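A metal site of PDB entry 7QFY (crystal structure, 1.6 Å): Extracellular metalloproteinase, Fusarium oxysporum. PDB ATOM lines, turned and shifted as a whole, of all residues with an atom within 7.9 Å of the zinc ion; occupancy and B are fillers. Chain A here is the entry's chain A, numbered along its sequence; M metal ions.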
ATOM      1  N   ASN A 147      16.851  -1.172  -3.598  1.00  0.00           N
ATOM      2  CA  ASN A 147      15.621  -1.952  -3.589  1.00  0.00           C
ATOM      3  C   ASN A 147      15.427  -2.540  -2.209  1.00  0.00           C
ATOM      4  O   ASN A 147      16.245  -2.351  -1.309  1.00  0.00           O
ATOM      5  CB  ASN A 147      15.636  -3.043  -4.671  1.00  0.00           C
ATOM      6  CG  ASN A 147      14.260  -3.286  -5.268  1.00  0.00           C
ATOM      7  OD1 ASN A 147      13.225  -2.946  -4.657  1.00  0.00           O
ATOM      8  ND2 ASN A 147      14.228  -3.836  -6.476  1.00  0.00           N
ATOM      9  N   ALA A 148      14.304  -3.218  -2.067  1.00  0.00           N
ATOM     10  CA  ALA A 148      13.970  -3.949  -0.857  1.00  0.00           C
ATOM     11  C   ALA A 148      13.043  -5.050  -1.302  1.00  0.00           C
ATOM     12  O   ALA A 148      12.423  -4.964  -2.367  1.00  0.00           O
ATOM     13  CB  ALA A 148      13.294  -3.061   0.187  1.00  0.00           C
ATOM     14  N   ASN A 149      12.939  -6.100  -0.489  1.00  0.00           N
ATOM     15  CA  ASN A 149      12.025  -7.162  -0.891  1.00  0.00           C
ATOM     16  C   ASN A 149      11.607  -7.984   0.301  1.00  0.00           C
ATOM     17  O   ASN A 149      12.116  -7.830   1.424  1.00  0.00           O
ATOM     18  CB  ASN A 149      12.639  -8.044  -1.958  1.00  0.00           C
ATOM     19  CG  ASN A 149      13.971  -8.523  -1.577  1.00  0.00           C
ATOM     20  OD1 ASN A 149      14.089  -9.370  -0.714  1.00  0.00           O
ATOM     21  ND2 ASN A 149      15.007  -7.972  -2.216  1.00  0.00           N
ATOM     22  N   PHE A 150      10.616  -8.828   0.069  1.00  0.00           N
ATOM     23  CA  PHE A 150      10.041  -9.656   1.113  1.00  0.00           C
ATOM     24  C   PHE A 150       9.647 -11.015   0.532  1.00  0.00           C
ATOM     25  O   PHE A 150       8.943 -11.077  -0.487  1.00  0.00           O
ATOM     26  CB  PHE A 150       8.823  -8.975   1.744  1.00  0.00           C
ATOM     27  CG  PHE A 150       8.428  -9.580   3.081  1.00  0.00           C
ATOM     28  CD1 PHE A 150       7.696 -10.754   3.147  1.00  0.00           C
ATOM     29  CD2 PHE A 150       8.813  -8.985   4.250  1.00  0.00           C
ATOM     30  CE1 PHE A 150       7.358 -11.316   4.366  1.00  0.00           C
ATOM     31  CE2 PHE A 150       8.475  -9.532   5.496  1.00  0.00           C
ATOM     32  CZ  PHE A 150       7.742 -10.693   5.544  1.00  0.00           C
ATOM     33  N   VAL A 181       8.842   2.167   3.456  1.00  0.00           N
ATOM     34  CA  VAL A 181       9.354   1.044   2.695  1.00  0.00           C
ATOM     35  C   VAL A 181       9.334  -0.232   3.528  1.00  0.00           C
ATOM     36  O   VAL A 181       8.937  -1.310   3.052  1.00  0.00           O
ATOM     37  CB  VAL A 181      10.774   1.346   2.192  1.00  0.00           C
ATOM     38  CG1 VAL A 181      11.291   0.116   1.427  1.00  0.00           C
ATOM     39  CG2 VAL A 181      10.791   2.587   1.318  1.00  0.00           C
ATOM     40  N   HIS A 184       5.778  -1.268   3.494  1.00  0.00           N
ATOM     41  CA  HIS A 184       5.474  -1.856   2.197  1.00  0.00           C
ATOM     42  C   HIS A 184       5.955  -3.312   2.130  1.00  0.00           C
ATOM     43  O   HIS A 184       5.194  -4.200   1.737  1.00  0.00           O
ATOM     44  CB  HIS A 184       6.101  -1.027   1.088  1.00  0.00           C
ATOM     45  CG  HIS A 184       6.022  -1.665  -0.254  1.00  0.00           C
ATOM     46  ND1 HIS A 184       5.146  -1.240  -1.229  1.00  0.00           N
ATOM     47  CD2 HIS A 184       6.691  -2.721  -0.780  1.00  0.00           C
ATOM     48  CE1 HIS A 184       5.293  -1.999  -2.303  1.00  0.00           C
ATOM     49  NE2 HIS A 184       6.216  -2.908  -2.060  1.00  0.00           N
ATOM     50  N   GLU A 185       7.192  -3.582   2.530  1.00  0.00           N
ATOM     51  CA  GLU A 185       7.720  -4.935   2.416  1.00  0.00           C
ATOM     52  C   GLU A 185       6.957  -5.903   3.319  1.00  0.00           C
ATOM     53  O   GLU A 185       6.554  -6.976   2.873  1.00  0.00           O
ATOM     54  CB  GLU A 185       9.200  -4.952   2.756  1.00  0.00           C
ATOM     55  CG  GLU A 185      10.092  -4.167   1.763  1.00  0.00           C
ATOM     56  CD  GLU A 185       9.812  -4.476   0.303  1.00  0.00           C
ATOM     57  OE1 GLU A 185       9.371  -5.596  -0.063  1.00  0.00           O
ATOM     58  OE2 GLU A 185      10.058  -3.563  -0.504  1.00  0.00           O
ATOM     59  N   TYR A 186       6.753  -5.527   4.574  1.00  0.00           N
ATOM     60  CA  TYR A 186       6.057  -6.396   5.519  1.00  0.00           C
ATOM     61  C   TYR A 186       4.639  -6.686   5.024  1.00  0.00           C
ATOM     62  O   TYR A 186       4.111  -7.786   5.210  1.00  0.00           O
ATOM     63  CB  TYR A 186       6.014  -5.730   6.902  1.00  0.00           C
ATOM     64  CG  TYR A 186       5.691  -6.639   8.086  1.00  0.00           C
ATOM     65  CD1 TYR A 186       4.414  -7.139   8.279  1.00  0.00           C
ATOM     66  CD2 TYR A 186       6.665  -6.986   9.007  1.00  0.00           C
ATOM     67  CE1 TYR A 186       4.107  -7.952   9.352  1.00  0.00           C
ATOM     68  CE2 TYR A 186       6.364  -7.793  10.091  1.00  0.00           C
ATOM     69  CZ  TYR A 186       5.080  -8.283  10.242  1.00  0.00           C
ATOM     70  OH  TYR A 186       4.768  -9.112  11.310  1.00  0.00           O
ATOM     71  N   THR A 187       4.030  -5.705   4.370  1.00  0.00           N
ATOM     72  CA  THR A 187       2.682  -5.902   3.840  1.00  0.00           C
ATOM     73  C   THR A 187       2.640  -6.987   2.772  1.00  0.00           C
ATOM     74  O   THR A 187       1.604  -7.627   2.589  1.00  0.00           O
ATOM     75  CB  THR A 187       2.139  -4.569   3.300  1.00  0.00           C
ATOM     76  OG1 THR A 187       2.158  -3.597   4.346  1.00  0.00           O
ATOM     77  CG2 THR A 187       0.716  -4.719   2.805  1.00  0.00           C
ATOM     78  N   HIS A 188       3.756  -7.247   2.079  1.00  0.00           N
ATOM     79  CA  HIS A 188       3.789  -8.412   1.190  1.00  0.00           C
ATOM     80  C   HIS A 188       3.575  -9.693   1.977  1.00  0.00           C
ATOM     81  O   HIS A 188       2.946 -10.641   1.480  1.00  0.00           O
ATOM     82  CB  HIS A 188       5.122  -8.470   0.442  1.00  0.00           C
ATOM     83  CG  HIS A 188       5.201  -7.558  -0.750  1.00  0.00           C
ATOM     84  ND1 HIS A 188       4.311  -7.627  -1.801  1.00  0.00           N
ATOM     85  CD2 HIS A 188       6.093  -6.588  -1.083  1.00  0.00           C
ATOM     86  CE1 HIS A 188       4.643  -6.732  -2.721  1.00  0.00           C
ATOM     87  NE2 HIS A 188       5.706  -6.083  -2.303  1.00  0.00           N
ATOM     88  N   GLY A 210      -0.403  -9.603  -8.594  1.00  0.00           N
ATOM     89  CA  GLY A 210       0.859  -9.105  -8.098  1.00  0.00           C
ATOM     90  C   GLY A 210       0.904  -7.593  -8.045  1.00  0.00           C
ATOM     91  O   GLY A 210       1.531  -7.029  -7.144  1.00  0.00           O
ATOM     92  N   GLY A 211       0.199  -6.935  -8.976  1.00  0.00           N
ATOM     93  CA  GLY A 211       0.068  -5.495  -8.932  1.00  0.00           C
ATOM     94  C   GLY A 211      -0.613  -5.009  -7.659  1.00  0.00           C
ATOM     95  O   GLY A 211      -0.115  -4.096  -6.979  1.00  0.00           O
ATOM     96  N   GLY A 213      -0.624  -6.649  -5.018  1.00  0.00           N
ATOM     97  CA  GLY A 213       0.417  -6.906  -4.028  1.00  0.00           C
ATOM     98  C   GLY A 213       1.301  -5.695  -3.765  1.00  0.00           C
ATOM     99  O   GLY A 213       1.614  -5.380  -2.621  1.00  0.00           O
ATOM    100  N   GLU A 214       1.717  -5.015  -4.833  1.00  0.00           N
ATOM    101  CA  GLU A 214       2.500  -3.789  -4.643  1.00  0.00           C
ATOM    102  C   GLU A 214       1.643  -2.671  -4.067  1.00  0.00           C
ATOM    103  O   GLU A 214       2.086  -1.937  -3.178  1.00  0.00           O
ATOM    104  CB  GLU A 214       3.132  -3.360  -5.960  1.00  0.00           C
ATOM    105  CG  GLU A 214       4.074  -4.417  -6.528  1.00  0.00           C
ATOM    106  CD  GLU A 214       5.186  -4.807  -5.577  1.00  0.00           C
ATOM    107  OE1 GLU A 214       5.590  -3.953  -4.771  1.00  0.00           O
ATOM    108  OE2 GLU A 214       5.609  -5.983  -5.602  1.00  0.00           O
ATOM    109  N   GLY A 215       0.397  -2.563  -4.541  1.00  0.00           N
ATOM    110  CA  GLY A 215      -0.444  -1.452  -4.130  1.00  0.00           C
ATOM    111  C   GLY A 215      -0.807  -1.488  -2.655  1.00  0.00           C
ATOM    112  O   GLY A 215      -0.830  -0.447  -1.991  1.00  0.00           O
ATOM    113  N   GLY A 217       0.878  -2.547  -0.129  1.00  0.00           N
ATOM    114  CA  GLY A 217       1.945  -2.032   0.714  1.00  0.00           C
ATOM    115  C   GLY A 217       2.058  -0.516   0.659  1.00  0.00           C
ATOM    116  O   GLY A 217       2.286   0.133   1.684  1.00  0.00           O
ATOM    117  N   ASP A 218       1.955   0.056  -0.551  1.00  0.00           N
ATOM    118  CA  ASP A 218       1.981   1.512  -0.674  1.00  0.00           C
ATOM    119  C   ASP A 218       0.814   2.120   0.077  1.00  0.00           C
ATOM    120  O   ASP A 218       0.956   3.145   0.743  1.00  0.00           O
ATOM    121  CB  ASP A 218       1.931   1.948  -2.148  1.00  0.00           C
ATOM    122  CG  ASP A 218       3.268   1.841  -2.881  1.00  0.00           C
ATOM    123  OD1 ASP A 218       4.190   1.165  -2.371  1.00  0.00           O
ATOM    124  OD2 ASP A 218       3.407   2.470  -3.975  1.00  0.00           O
ATOM    125  N   ILE A 249       8.882   7.021  -5.608  1.00  0.00           N
ATOM    126  CA  ILE A 249       9.261   5.942  -6.501  1.00  0.00           C
ATOM    127  C   ILE A 249       8.174   5.588  -7.509  1.00  0.00           C
ATOM    128  O   ILE A 249       8.419   4.734  -8.381  1.00  0.00           O
ATOM    129  CB  ILE A 249       9.663   4.671  -5.725  1.00  0.00           C
ATOM    130  CG1 ILE A 249       8.524   4.150  -4.820  1.00  0.00           C
ATOM    131  CG2 ILE A 249      10.937   4.912  -4.939  1.00  0.00           C
ATOM    132  CD1 ILE A 249       8.952   2.933  -3.981  1.00  0.00           C
ATOM    133  N   ARG A 250       6.987   6.197  -7.435  1.00  0.00           N
ATOM    134  CA  ARG A 250       5.895   5.887  -8.362  1.00  0.00           C
ATOM    135  C   ARG A 250       5.629   7.049  -9.309  1.00  0.00           C
ATOM    136  O   ARG A 250       6.081   8.175  -9.104  1.00  0.00           O
ATOM    137  CB  ARG A 250       4.604   5.531  -7.596  1.00  0.00           C
ATOM    138  CG  ARG A 250       4.762   4.564  -6.443  1.00  0.00           C
ATOM    139  CD  ARG A 250       5.385   3.235  -6.827  1.00  0.00           C
ATOM    140  NE  ARG A 250       5.404   2.316  -5.693  1.00  0.00           N
ATOM    141  CZ  ARG A 250       6.281   1.342  -5.502  1.00  0.00           C
ATOM    142  NH1 ARG A 250       7.255   1.108  -6.379  1.00  0.00           N
ATOM    143  NH2 ARG A 250       6.206   0.588  -4.408  1.00  0.00           N
ATOM    144  N   VAL A 274       4.290  -4.931 -12.156  1.00  0.00           N
ATOM    145  CA  VAL A 274       3.447  -4.940 -10.958  1.00  0.00           C
ATOM    146  C   VAL A 274       3.524  -3.611 -10.183  1.00  0.00           C
ATOM    147  O   VAL A 274       2.544  -3.233  -9.528  1.00  0.00           O
ATOM    148  CB  VAL A 274       3.796  -6.118 -10.035  1.00  0.00           C
ATOM    149  CG1 VAL A 274       3.415  -7.419 -10.687  1.00  0.00           C
ATOM    150  CG2 VAL A 274       5.293  -6.117  -9.629  1.00  0.00           C
ATOM    151  N   HIS A 275       4.651  -2.890 -10.230  1.00  0.00           N
ATOM    152  CA  HIS A 275       4.693  -1.644  -9.461  1.00  0.00           C
ATOM    153  C   HIS A 275       3.838  -0.566 -10.123  1.00  0.00           C
ATOM    154  O   HIS A 275       3.175   0.212  -9.425  1.00  0.00           O
ATOM    155  CB  HIS A 275       6.141  -1.184  -9.281  1.00  0.00           C
ATOM    156  CG  HIS A 275       6.978  -2.155  -8.527  1.00  0.00           C
ATOM    157  ND1 HIS A 275       7.780  -3.091  -9.150  1.00  0.00           N
ATOM    158  CD2 HIS A 275       7.107  -2.383  -7.198  1.00  0.00           C
ATOM    159  CE1 HIS A 275       8.384  -3.826  -8.225  1.00  0.00           C
ATOM    160  NE2 HIS A 275       7.987  -3.419  -7.034  1.00  0.00           N
HETATM  161 ZN    ZN M   1       6.629  -4.552  -3.199  1.00  0.00          ZN
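The side-chain carboxylate (OE1) of Glu 214 sits close to a ring nitrogen (NE2) of His 275 (3.3 Å).
ND1 of His 184 is in hydrogen-bond range of OD1 of Asp 218, 2.8 Å away.
Three residues have an atom within 4 Å of the zinc ion: His 184, His 188 and Glu 214.
The nearest printed residue that does not touch the zinc ion is His 275 (4.2 Å).
The zinc ion is bound by the side-chain carboxylate (OE1) of Glu 214 (2.0 Å), a ring nitrogen (NE2) of His 188 (2.0 Å) and a ring nitrogen (NE2) of His 184 (2.0 Å).
The zinc ion has three donor atoms within binding distance.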
